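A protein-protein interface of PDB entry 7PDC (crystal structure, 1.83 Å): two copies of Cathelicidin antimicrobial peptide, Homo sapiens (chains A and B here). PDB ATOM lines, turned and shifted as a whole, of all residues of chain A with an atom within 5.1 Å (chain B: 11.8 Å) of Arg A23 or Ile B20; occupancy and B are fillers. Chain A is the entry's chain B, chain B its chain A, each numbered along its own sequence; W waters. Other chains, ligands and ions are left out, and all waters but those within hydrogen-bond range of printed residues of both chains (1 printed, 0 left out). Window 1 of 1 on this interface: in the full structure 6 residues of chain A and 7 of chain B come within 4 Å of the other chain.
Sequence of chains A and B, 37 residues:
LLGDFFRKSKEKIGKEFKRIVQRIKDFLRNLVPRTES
Water W1 lies within hydrogen-bond range of O of Arg A23 (2.7 Å), OE2 of Glu B16 (2.8 Å) and N of Phe A27 (3.4 Å).
OE2 of Glu B16 lies within salt-bridge range of NH1 of Arg A23 (2.8 Å).
Of chain B, only Glu B16, Arg B19, Ile B20 and Arg B23 come within 4 Å of Arg A23. Of the printed residues of chain A, Ile B20 touches Arg A23 (3.7 Å), Ile A24 (3.7 Å) and Phe A27 (3.7 Å). Ile A20 touches three residues of chain B. No residue of chain B comes within 4 Å of Val A21. No residue of chain B comes within 4 Å of Gln A22. Of chain B, only Ile B13, Glu B16 and Ile B20 come within 4 Å of Phe A27. Printed residues of chain A within 4 Å of Arg B19: Arg A23 (3.9 Å). Of the printed residues of chain A, Arg B23 touches Ile A20 (3.8 Å) and Arg A23 (3.5 Å). Of the printed residues of chain A, Ile B24 touches Ile A20 and Ile A24. Of the printed residues of chain A, Glu B16 touches Arg A23 (2.8 Å) and Phe A27 (3.5 Å). Of the printed residues of chain A, Phe B27 touches Ile A20. Lys B15 touches none of the printed residues of chain A. Lys B18 touches none of the printed residues of chain A. The nearest residue of chain B that does not touch Arg A23 is Val B21 (6.9 Å). The nearest printed residue of chain A that does not touch Phe B27 is Lys A18 (6.3 Å).
Hydrophobic or aromatic side chains of chain B that line the printed part of chain A: Ile B13, Ile B20, Ile B24 and Phe B27. Printed residues of chain A that touch a printed residue of chain B: Ile A20, Arg A23, Ile A24 and Phe A27. Hydrophobic or aromatic side chains of chain A that line the printed part of chain B: Ile A20, Ile A24 and Phe A27. Among the printed residues, 12 pairs touch across the chains. Among the printed residues, Asp or Glu carboxylates within 4 Å of a Lys or Arg side-chain nitrogen of the other chain: Arg A23 with Glu B16 (2.8 Å).
Among the printed residues, pairs that only touch across the chains: Ile A20 with Arg B23 (3.8 Å), Ile A20 with Ile B24 (3.9 Å), Ile A20 with Phe B27 (3.6 Å), Arg A23 with Arg B19 (3.9 Å), Arg A23 with Ile B20 (3.7 Å), Arg A23 with Arg B23 (3.5 Å), Ile A24 with Ile B20 (3.7 Å), Ile A24 with Ile B24 (3.9 Å), Phe A27 with Ile B13 (3.6 Å), Phe A27 with Glu B16 (3.5 Å) and Phe A27 with Ile B20 (3.7 Å).
The side-chain carboxylate (OE1) of Glu B16 lies within salt-bridge range of the guanidinium group (NH1) of Arg B19 (3.1 Å). The guanidinium group (NH1) of Arg B23 lies close to the backbone carbonyl oxygen (O) of Arg B19, 3.2 Å away.
Ile A20 touches Arg B23, and with the chains exchanged Arg A23 touches Ile B20. Ile A20 touches Ile B24, and with the chains exchanged Ile A24 touches Ile B20. Arg B23 touches its own counterpart, Arg A23. Ile B24 touches its own counterpart, Ile A24. 10 positions are printed for both chains. Of the 12 pairs that touch across the chains among the printed residues, 8 have their exchanged pair printed and touching as well.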
ATOM      1  N   LYS A  18      20.847 -20.840  22.985  1.00  0.00           N
ATOM      2  CA  LYS A  18      20.562 -20.453  21.594  1.00  0.00           C
ATOM      3  C   LYS A  18      20.998 -19.001  21.293  1.00  0.00           C
ATOM      4  O   LYS A  18      21.651 -18.756  20.267  1.00  0.00           O
ATOM      5  CB  LYS A  18      19.068 -20.665  21.275  1.00  0.00           C
ATOM      6  CG  LYS A  18      18.775 -22.114  20.901  1.00  0.00           C
ATOM      7  CD  LYS A  18      17.292 -22.460  21.006  1.00  0.00           C
ATOM      8  CE  LYS A  18      17.056 -23.954  21.068  1.00  0.00           C
ATOM      9  NZ  LYS A  18      17.372 -24.527  22.406  1.00  0.00           N
ATOM     10  N   ARG A  19      20.685 -18.066  22.216  1.00  0.00           N
ATOM     11  CA  ARG A  19      21.035 -16.640  22.127  1.00  0.00           C
ATOM     12  C   ARG A  19      22.557 -16.431  22.051  1.00  0.00           C
ATOM     13  O   ARG A  19      23.010 -15.615  21.243  1.00  0.00           O
ATOM     14  CB  ARG A  19      20.458 -15.855  23.320  1.00  0.00           C
ATOM     15  CG  ARG A  19      19.002 -15.450  23.128  1.00  0.00           C
ATOM     16  CD  ARG A  19      18.434 -14.823  24.390  1.00  0.00           C
ATOM     17  NE  ARG A  19      17.023 -14.460  24.242  1.00  0.00           N
ATOM     18  CZ  ARG A  19      16.140 -14.423  25.238  1.00  0.00           C
ATOM     19  NH1 ARG A  19      16.508 -14.734  26.476  1.00  0.00           N
ATOM     20  NH2 ARG A  19      14.880 -14.083  25.004  1.00  0.00           N
ATOM     21  N   ILE A  20      23.332 -17.159  22.880  1.00  0.00           N
ATOM     22  CA  ILE A  20      24.807 -17.048  22.901  1.00  0.00           C
ATOM     23  C   ILE A  20      25.427 -17.646  21.613  1.00  0.00           C
ATOM     24  O   ILE A  20      26.326 -17.034  21.024  1.00  0.00           O
ATOM     25  CB  ILE A  20      25.447 -17.611  24.202  1.00  0.00           C
ATOM     26  CG1 ILE A  20      24.910 -16.872  25.460  1.00  0.00           C
ATOM     27  CG2 ILE A  20      26.991 -17.526  24.140  1.00  0.00           C
ATOM     28  CD1 ILE A  20      24.862 -17.702  26.679  1.00  0.00           C
ATOM     29  N   VAL A  21      24.931 -18.845  21.192  1.00  0.00           N
ATOM     30  CA  VAL A  21      25.341 -19.538  19.960  1.00  0.00           C
ATOM     31  C   VAL A  21      25.150 -18.574  18.762  1.00  0.00           C
ATOM     32  O   VAL A  21      26.086 -18.388  17.979  1.00  0.00           O
ATOM     33  CB  VAL A  21      24.597 -20.897  19.778  1.00  0.00           C
ATOM     34  CG1 VAL A  21      24.810 -21.467  18.370  1.00  0.00           C
ATOM     35  CG2 VAL A  21      25.051 -21.919  20.826  1.00  0.00           C
ATOM     36  N   GLN A  22      23.958 -17.936  18.663  1.00  0.00           N
ATOM     37  CA  GLN A  22      23.609 -16.955  17.622  1.00  0.00           C
ATOM     38  C   GLN A  22      24.604 -15.774  17.617  1.00  0.00           C
ATOM     39  O   GLN A  22      25.113 -15.418  16.554  1.00  0.00           O
ATOM     40  CB  GLN A  22      22.154 -16.448  17.824  1.00  0.00           C
ATOM     41  CG  GLN A  22      21.688 -15.439  16.778  1.00  0.00           C
ATOM     42  CD  GLN A  22      20.241 -15.022  16.947  1.00  0.00           C
ATOM     43  OE1 GLN A  22      19.868 -14.329  17.904  1.00  0.00           O
ATOM     44  NE2 GLN A  22      19.402 -15.386  15.981  1.00  0.00           N
ATOM     45  N   ARG A  23      24.854 -15.171  18.795  1.00  0.00           N
ATOM     46  CA  ARG A  23      25.755 -14.031  18.970  1.00  0.00           C
ATOM     47  C   ARG A  23      27.193 -14.401  18.525  1.00  0.00           C
ATOM     48  O   ARG A  23      27.804 -13.628  17.783  1.00  0.00           O
ATOM     49  CB  ARG A  23      25.723 -13.529  20.420  1.00  0.00           C
ATOM     50  CG  ARG A  23      26.623 -12.318  20.665  1.00  0.00           C
ATOM     51  CD  ARG A  23      26.484 -11.726  22.082  1.00  0.00           C
ATOM     52  NE  ARG A  23      25.162 -11.137  22.318  1.00  0.00           N
ATOM     53  CZ  ARG A  23      24.766  -9.925  21.938  1.00  0.00           C
ATOM     54  NH1 ARG A  23      25.592  -9.123  21.271  1.00  0.00           N
ATOM     55  NH2 ARG A  23      23.537  -9.505  22.217  1.00  0.00           N
ATOM     56  N   ILE A  24      27.706 -15.571  18.960  1.00  0.00           N
ATOM     57  CA  ILE A  24      29.037 -16.064  18.561  1.00  0.00           C
ATOM     58  C   ILE A  24      29.120 -16.228  17.022  1.00  0.00           C
ATOM     59  O   ILE A  24      30.082 -15.737  16.409  1.00  0.00           O
ATOM     60  CB  ILE A  24      29.482 -17.317  19.362  1.00  0.00           C
ATOM     61  CG1 ILE A  24      29.724 -16.939  20.860  1.00  0.00           C
ATOM     62  CG2 ILE A  24      30.759 -17.968  18.755  1.00  0.00           C
ATOM     63  CD1 ILE A  24      29.865 -18.139  21.833  1.00  0.00           C
ATOM     64  N   LYS A  25      28.087 -16.856  16.402  1.00  0.00           N
ATOM     65  CA  LYS A  25      28.000 -17.050  14.943  1.00  0.00           C
ATOM     66  C   LYS A  25      28.098 -15.717  14.189  1.00  0.00           C
ATOM     67  O   LYS A  25      28.903 -15.600  13.267  1.00  0.00           O
ATOM     68  CB  LYS A  25      26.693 -17.772  14.572  1.00  0.00           C
ATOM     69  CG  LYS A  25      26.741 -19.283  14.744  1.00  0.00           C
ATOM     70  CD  LYS A  25      25.345 -19.864  14.965  1.00  0.00           C
ATOM     71  CE  LYS A  25      24.734 -20.463  13.721  1.00  0.00           C
ATOM     72  NZ  LYS A  25      23.358 -20.970  13.975  1.00  0.00           N
ATOM     73  N   ASP A  26      27.279 -14.715  14.602  1.00  0.00           N
ATOM     74  CA  ASP A  26      27.237 -13.361  14.047  1.00  0.00           C
ATOM     75  C   ASP A  26      28.621 -12.675  14.083  1.00  0.00           C
ATOM     76  O   ASP A  26      29.028 -12.045  13.107  1.00  0.00           O
ATOM     77  CB  ASP A  26      26.231 -12.520  14.838  1.00  0.00           C
ATOM     78  CG  ASP A  26      24.779 -12.816  14.536  1.00  0.00           C
ATOM     79  OD1 ASP A  26      24.512 -13.708  13.689  1.00  0.00           O
ATOM     80  OD2 ASP A  26      23.906 -12.152  15.138  1.00  0.00           O
ATOM     81  N   PHE A  27      29.307 -12.780  15.221  1.00  0.00           N
ATOM     82  CA  PHE A  27      30.638 -12.233  15.449  1.00  0.00           C
ATOM     83  C   PHE A  27      31.648 -12.876  14.493  1.00  0.00           C
ATOM     84  O   PHE A  27      32.345 -12.155  13.775  1.00  0.00           O
ATOM     85  CB  PHE A  27      31.043 -12.469  16.916  1.00  0.00           C
ATOM     86  CG  PHE A  27      32.352 -11.846  17.326  1.00  0.00           C
ATOM     87  CD1 PHE A  27      32.454 -10.475  17.532  1.00  0.00           C
ATOM     88  CD2 PHE A  27      33.486 -12.628  17.509  1.00  0.00           C
ATOM     89  CE1 PHE A  27      33.664  -9.901  17.934  1.00  0.00           C
ATOM     90  CE2 PHE A  27      34.697 -12.055  17.899  1.00  0.00           C
ATOM     91  CZ  PHE A  27      34.772 -10.697  18.124  1.00  0.00           C
ATOM     92  N   GLU B  11      37.526  -0.907  18.545  1.00  0.00           N
ATOM     93  CA  GLU B  11      36.738  -0.659  19.761  1.00  0.00           C
ATOM     94  C   GLU B  11      35.431  -1.445  19.748  1.00  0.00           C
ATOM     95  O   GLU B  11      35.133  -2.130  20.730  1.00  0.00           O
ATOM     96  CB  GLU B  11      36.465   0.835  19.950  1.00  0.00           C
ATOM     97  CG  GLU B  11      37.603   1.554  20.656  1.00  0.00           C
ATOM     98  CD  GLU B  11      37.606   3.068  20.553  1.00  0.00           C
ATOM     99  OE1 GLU B  11      36.513   3.674  20.451  1.00  0.00           O
ATOM    100  OE2 GLU B  11      38.711   3.652  20.603  1.00  0.00           O
ATOM    101  N   LYS B  12      34.688  -1.385  18.620  1.00  0.00           N
ATOM    102  CA  LYS B  12      33.434  -2.123  18.422  1.00  0.00           C
ATOM    103  C   LYS B  12      33.662  -3.644  18.489  1.00  0.00           C
ATOM    104  O   LYS B  12      32.833  -4.361  19.050  1.00  0.00           O
ATOM    105  CB  LYS B  12      32.787  -1.730  17.092  1.00  0.00           C
ATOM    106  CG  LYS B  12      32.024  -0.407  17.152  1.00  0.00           C
ATOM    107  CD  LYS B  12      31.436  -0.043  15.791  1.00  0.00           C
ATOM    108  CE  LYS B  12      30.747   1.303  15.776  1.00  0.00           C
ATOM    109  NZ  LYS B  12      29.412   1.261  16.435  1.00  0.00           N
ATOM    110  N   ILE B  13      34.790  -4.131  17.929  1.00  0.00           N
ATOM    111  CA  ILE B  13      35.117  -5.565  17.954  1.00  0.00           C
ATOM    112  C   ILE B  13      35.392  -6.022  19.388  1.00  0.00           C
ATOM    113  O   ILE B  13      34.842  -7.039  19.815  1.00  0.00           O
ATOM    114  CB  ILE B  13      36.227  -5.943  16.923  1.00  0.00           C
ATOM    115  CG1 ILE B  13      35.681  -5.812  15.479  1.00  0.00           C
ATOM    116  CG2 ILE B  13      36.763  -7.364  17.165  1.00  0.00           C
ATOM    117  CD1 ILE B  13      36.769  -5.575  14.386  1.00  0.00           C
ATOM    118  N   GLY B  14      36.199  -5.242  20.116  1.00  0.00           N
ATOM    119  CA  GLY B  14      36.541  -5.493  21.515  1.00  0.00           C
ATOM    120  C   GLY B  14      35.331  -5.533  22.429  1.00  0.00           C
ATOM    121  O   GLY B  14      35.221  -6.427  23.271  1.00  0.00           O
ATOM    122  N   LYS B  15      34.402  -4.572  22.253  1.00  0.00           N
ATOM    123  CA  LYS B  15      33.166  -4.481  23.016  1.00  0.00           C
ATOM    124  C   LYS B  15      32.275  -5.707  22.778  1.00  0.00           C
ATOM    125  O   LYS B  15      31.747  -6.266  23.746  1.00  0.00           O
ATOM    126  CB  LYS B  15      32.412  -3.179  22.726  1.00  0.00           C
ATOM    127  CG  LYS B  15      33.036  -1.974  23.402  1.00  0.00           C
ATOM    128  CD  LYS B  15      32.111  -0.762  23.327  1.00  0.00           C
ATOM    129  CE  LYS B  15      32.742   0.464  23.945  1.00  0.00           C
ATOM    130  NZ  LYS B  15      32.073   1.708  23.485  1.00  0.00           N
ATOM    131  N   GLU B  16      32.159  -6.155  21.502  1.00  0.00           N
ATOM    132  CA  GLU B  16      31.376  -7.349  21.169  1.00  0.00           C
ATOM    133  C   GLU B  16      32.015  -8.614  21.771  1.00  0.00           C
ATOM    134  O   GLU B  16      31.284  -9.514  22.206  1.00  0.00           O
ATOM    135  CB  GLU B  16      31.168  -7.482  19.645  1.00  0.00           C
ATOM    136  CG  GLU B  16      30.137  -8.538  19.247  1.00  0.00           C
ATOM    137  CD  GLU B  16      28.747  -8.435  19.857  1.00  0.00           C
ATOM    138  OE1 GLU B  16      28.313  -7.309  20.196  1.00  0.00           O
ATOM    139  OE2 GLU B  16      28.093  -9.493  20.002  1.00  0.00           O
ATOM    140  N   PHE B  17      33.367  -8.666  21.823  1.00  0.00           N
ATOM    141  CA  PHE B  17      34.086  -9.793  22.440  1.00  0.00           C
ATOM    142  C   PHE B  17      33.760  -9.823  23.955  1.00  0.00           C
ATOM    143  O   PHE B  17      33.468 -10.898  24.498  1.00  0.00           O
ATOM    144  CB  PHE B  17      35.609  -9.706  22.199  1.00  0.00           C
ATOM    145  CG  PHE B  17      36.396 -10.871  22.769  1.00  0.00           C
ATOM    146  CD1 PHE B  17      36.514 -12.065  22.065  1.00  0.00           C
ATOM    147  CD2 PHE B  17      37.022 -10.768  24.012  1.00  0.00           C
ATOM    148  CE1 PHE B  17      37.249 -13.141  22.587  1.00  0.00           C
ATOM    149  CE2 PHE B  17      37.753 -11.846  24.538  1.00  0.00           C
ATOM    150  CZ  PHE B  17      37.861 -13.026  23.819  1.00  0.00           C
ATOM    151  N   LYS B  18      33.746  -8.630  24.613  1.00  0.00           N
ATOM    152  CA  LYS B  18      33.382  -8.497  26.041  1.00  0.00           C
ATOM    153  C   LYS B  18      31.915  -8.943  26.256  1.00  0.00           C
ATOM    154  O   LYS B  18      31.619  -9.614  27.255  1.00  0.00           O
ATOM    155  CB  LYS B  18      33.587  -7.050  26.528  1.00  0.00           C
ATOM    156  CG  LYS B  18      33.449  -6.887  28.043  1.00  0.00           C
ATOM    157  CD  LYS B  18      33.559  -5.432  28.485  1.00  0.00           C
ATOM    158  CE  LYS B  18      33.455  -5.299  29.986  1.00  0.00           C
ATOM    159  NZ  LYS B  18      33.421  -3.876  30.412  1.00  0.00           N
ATOM    160  N   ARG B  19      31.003  -8.569  25.321  1.00  0.00           N
ATOM    161  CA  ARG B  19      29.583  -8.962  25.397  1.00  0.00           C
ATOM    162  C   ARG B  19      29.446 -10.495  25.423  1.00  0.00           C
ATOM    163  O   ARG B  19      28.746 -11.039  26.274  1.00  0.00           O
ATOM    164  CB  ARG B  19      28.791  -8.380  24.232  1.00  0.00           C
ATOM    165  CG  ARG B  19      28.227  -7.021  24.554  1.00  0.00           C
ATOM    166  CD  ARG B  19      27.349  -6.465  23.460  1.00  0.00           C
ATOM    167  NE  ARG B  19      27.357  -5.013  23.593  1.00  0.00           N
ATOM    168  CZ  ARG B  19      28.072  -4.194  22.834  1.00  0.00           C
ATOM    169  NH1 ARG B  19      28.763  -4.667  21.800  1.00  0.00           N
ATOM    170  NH2 ARG B  19      28.070  -2.888  23.074  1.00  0.00           N
ATOM    171  N   ILE B  20      30.151 -11.172  24.518  1.00  0.00           N
ATOM    172  CA  ILE B  20      30.144 -12.639  24.446  1.00  0.00           C
ATOM    173  C   ILE B  20      30.671 -13.282  25.743  1.00  0.00           C
ATOM    174  O   ILE B  20      30.024 -14.190  26.256  1.00  0.00           O
ATOM    175  CB  ILE B  20      30.896 -13.131  23.184  1.00  0.00           C
ATOM    176  CG1 ILE B  20      30.091 -12.809  21.903  1.00  0.00           C
ATOM    177  CG2 ILE B  20      31.206 -14.634  23.273  1.00  0.00           C
ATOM    178  CD1 ILE B  20      30.951 -12.734  20.580  1.00  0.00           C
ATOM    179  N   VAL B  21      31.849 -12.824  26.253  1.00  0.00           N
ATOM    180  CA  VAL B  21      32.503 -13.345  27.472  1.00  0.00           C
ATOM    181  C   VAL B  21      31.569 -13.163  28.689  1.00  0.00           C
ATOM    182  O   VAL B  21      31.408 -14.098  29.476  1.00  0.00           O
ATOM    183  CB  VAL B  21      33.904 -12.702  27.721  1.00  0.00           C
ATOM    184  CG1 VAL B  21      34.495 -13.147  29.062  1.00  0.00           C
ATOM    185  CG2 VAL B  21      34.872 -13.005  26.582  1.00  0.00           C
ATOM    186  N   GLN B  22      30.945 -11.966  28.823  1.00  0.00           N
ATOM    187  CA  GLN B  22      30.001 -11.686  29.911  1.00  0.00           C
ATOM    188  C   GLN B  22      28.794 -12.632  29.871  1.00  0.00           C
ATOM    189  O   GLN B  22      28.435 -13.193  30.910  1.00  0.00           O
ATOM    190  CB  GLN B  22      29.563 -10.204  29.910  1.00  0.00           C
ATOM    191  CG  GLN B  22      28.916  -9.754  31.226  1.00  0.00           C
ATOM    192  CD  GLN B  22      28.767  -8.248  31.331  1.00  0.00           C
ATOM    193  OE1 GLN B  22      28.187  -7.582  30.461  1.00  0.00           O
ATOM    194  NE2 GLN B  22      29.259  -7.681  32.425  1.00  0.00           N
ATOM    195  N   ARG B  23      28.215 -12.863  28.672  1.00  0.00           N
ATOM    196  CA  ARG B  23      27.070 -13.776  28.478  1.00  0.00           C
ATOM    197  C   ARG B  23      27.476 -15.234  28.820  1.00  0.00           C
ATOM    198  O   ARG B  23      26.703 -15.965  29.457  1.00  0.00           O
ATOM    199  CB  ARG B  23      26.603 -13.774  27.019  1.00  0.00           C
ATOM    200  CG  ARG B  23      26.016 -12.483  26.422  1.00  0.00           C
ATOM    201  CD  ARG B  23      25.161 -11.664  27.337  1.00  0.00           C
ATOM    202  NE  ARG B  23      24.421 -10.640  26.592  1.00  0.00           N
ATOM    203  CZ  ARG B  23      24.914  -9.465  26.209  1.00  0.00           C
ATOM    204  NH1 ARG B  23      26.186  -9.158  26.446  1.00  0.00           N
ATOM    205  NH2 ARG B  23      24.152  -8.604  25.551  1.00  0.00           N
ATOM    206  N   ILE B  24      28.675 -15.651  28.369  1.00  0.00           N
ATOM    207  CA  ILE B  24      29.174 -17.001  28.642  1.00  0.00           C
ATOM    208  C   ILE B  24      29.307 -17.228  30.155  1.00  0.00           C
ATOM    209  O   ILE B  24      28.757 -18.200  30.676  1.00  0.00           O
ATOM    210  CB  ILE B  24      30.466 -17.332  27.863  1.00  0.00           C
ATOM    211  CG1 ILE B  24      30.157 -17.558  26.356  1.00  0.00           C
ATOM    212  CG2 ILE B  24      31.127 -18.575  28.463  1.00  0.00           C
ATOM    213  CD1 ILE B  24      31.382 -17.617  25.438  1.00  0.00           C
ATOM    214  N   LYS B  25      30.003 -16.314  30.851  1.00  0.00           N
ATOM    215  CA  LYS B  25      30.197 -16.387  32.304  1.00  0.00           C
ATOM    216  C   LYS B  25      28.863 -16.512  33.027  1.00  0.00           C
ATOM    217  O   LYS B  25      28.674 -17.451  33.813  1.00  0.00           O
ATOM    218  CB  LYS B  25      30.984 -15.165  32.813  1.00  0.00           C
ATOM    219  CG  LYS B  25      32.478 -15.249  32.527  1.00  0.00           C
ATOM    220  CD  LYS B  25      33.112 -13.867  32.566  1.00  0.00           C
ATOM    221  CE  LYS B  25      33.953 -13.650  33.797  1.00  0.00           C
ATOM    222  NZ  LYS B  25      34.711 -12.376  33.719  1.00  0.00           N
ATOM    223  N   ASP B  26      27.927 -15.589  32.727  1.00  0.00           N
ATOM    224  CA  ASP B  26      26.573 -15.562  33.296  1.00  0.00           C
ATOM    225  C   ASP B  26      25.877 -16.917  33.069  1.00  0.00           C
ATOM    226  O   ASP B  26      25.431 -17.509  34.045  1.00  0.00           O
ATOM    227  CB  ASP B  26      25.761 -14.378  32.726  1.00  0.00           C
ATOM    228  CG  ASP B  26      24.331 -14.218  33.234  1.00  0.00           C
ATOM    229  OD1 ASP B  26      23.968 -14.881  34.228  1.00  0.00           O
ATOM    230  OD2 ASP B  26      23.579 -13.413  32.644  1.00  0.00           O
ATOM    231  N   PHE B  27      25.857 -17.436  31.816  1.00  0.00           N
ATOM    232  CA  PHE B  27      25.269 -18.744  31.490  1.00  0.00           C
ATOM    233  C   PHE B  27      25.871 -19.872  32.348  1.00  0.00           C
ATOM    234  O   PHE B  27      25.131 -20.590  33.009  1.00  0.00           O
ATOM    235  CB  PHE B  27      25.424 -19.073  29.981  1.00  0.00           C
ATOM    236  CG  PHE B  27      24.846 -20.390  29.505  1.00  0.00           C
ATOM    237  CD1 PHE B  27      23.480 -20.529  29.274  1.00  0.00           C
ATOM    238  CD2 PHE B  27      25.677 -21.482  29.241  1.00  0.00           C
ATOM    239  CE1 PHE B  27      22.948 -21.746  28.820  1.00  0.00           C
ATOM    240  CE2 PHE B  27      25.143 -22.695  28.776  1.00  0.00           C
ATOM    241  CZ  PHE B  27      23.781 -22.821  28.579  1.00  0.00           C
ATOM    242  N   LEU B  28      27.208 -19.993  32.364  1.00  0.00           N
ATOM    243  CA  LEU B  28      27.918 -21.035  33.110  1.00  0.00           C
ATOM    244  C   LEU B  28      27.710 -21.018  34.623  1.00  0.00           C
ATOM    245  O   LEU B  28      27.570 -22.086  35.231  1.00  0.00           O
ATOM    246  CB  LEU B  28      29.424 -20.988  32.789  1.00  0.00           C
ATOM    247  CG  LEU B  28      29.865 -21.333  31.352  1.00  0.00           C
ATOM    248  CD1 LEU B  28      31.357 -21.158  31.215  1.00  0.00           C
ATOM    249  CD2 LEU B  28      29.453 -22.761  30.945  1.00  0.00           C
ATOM    250  N   ARG B  29      27.688 -19.819  35.228  1.00  0.00           N
ATOM    251  CA  ARG B  29      27.534 -19.639  36.676  1.00  0.00           C
ATOM    252  C   ARG B  29      26.071 -19.783  37.161  1.00  0.00           C
ATOM    253  O   ARG B  29      25.811 -20.416  38.189  1.00  0.00           O
ATOM    254  CB  ARG B  29      28.125 -18.277  37.097  1.00  0.00           C
ATOM    255  CG  ARG B  29      29.649 -18.208  36.975  1.00  0.00           C
ATOM    256  CD  ARG B  29      30.199 -16.788  36.883  1.00  0.00           C
ATOM    257  NE  ARG B  29      31.656 -16.806  36.727  1.00  0.00           N
ATOM    258  CZ  ARG B  29      32.425 -15.730  36.566  1.00  0.00           C
ATOM    259  NH1 ARG B  29      31.886 -14.517  36.527  1.00  0.00           N
ATOM    260  NH2 ARG B  29      33.740 -15.860  36.445  1.00  0.00           N
HETATM  261  O   HOH W   1      27.731 -10.917  17.645  1.00  0.00           O
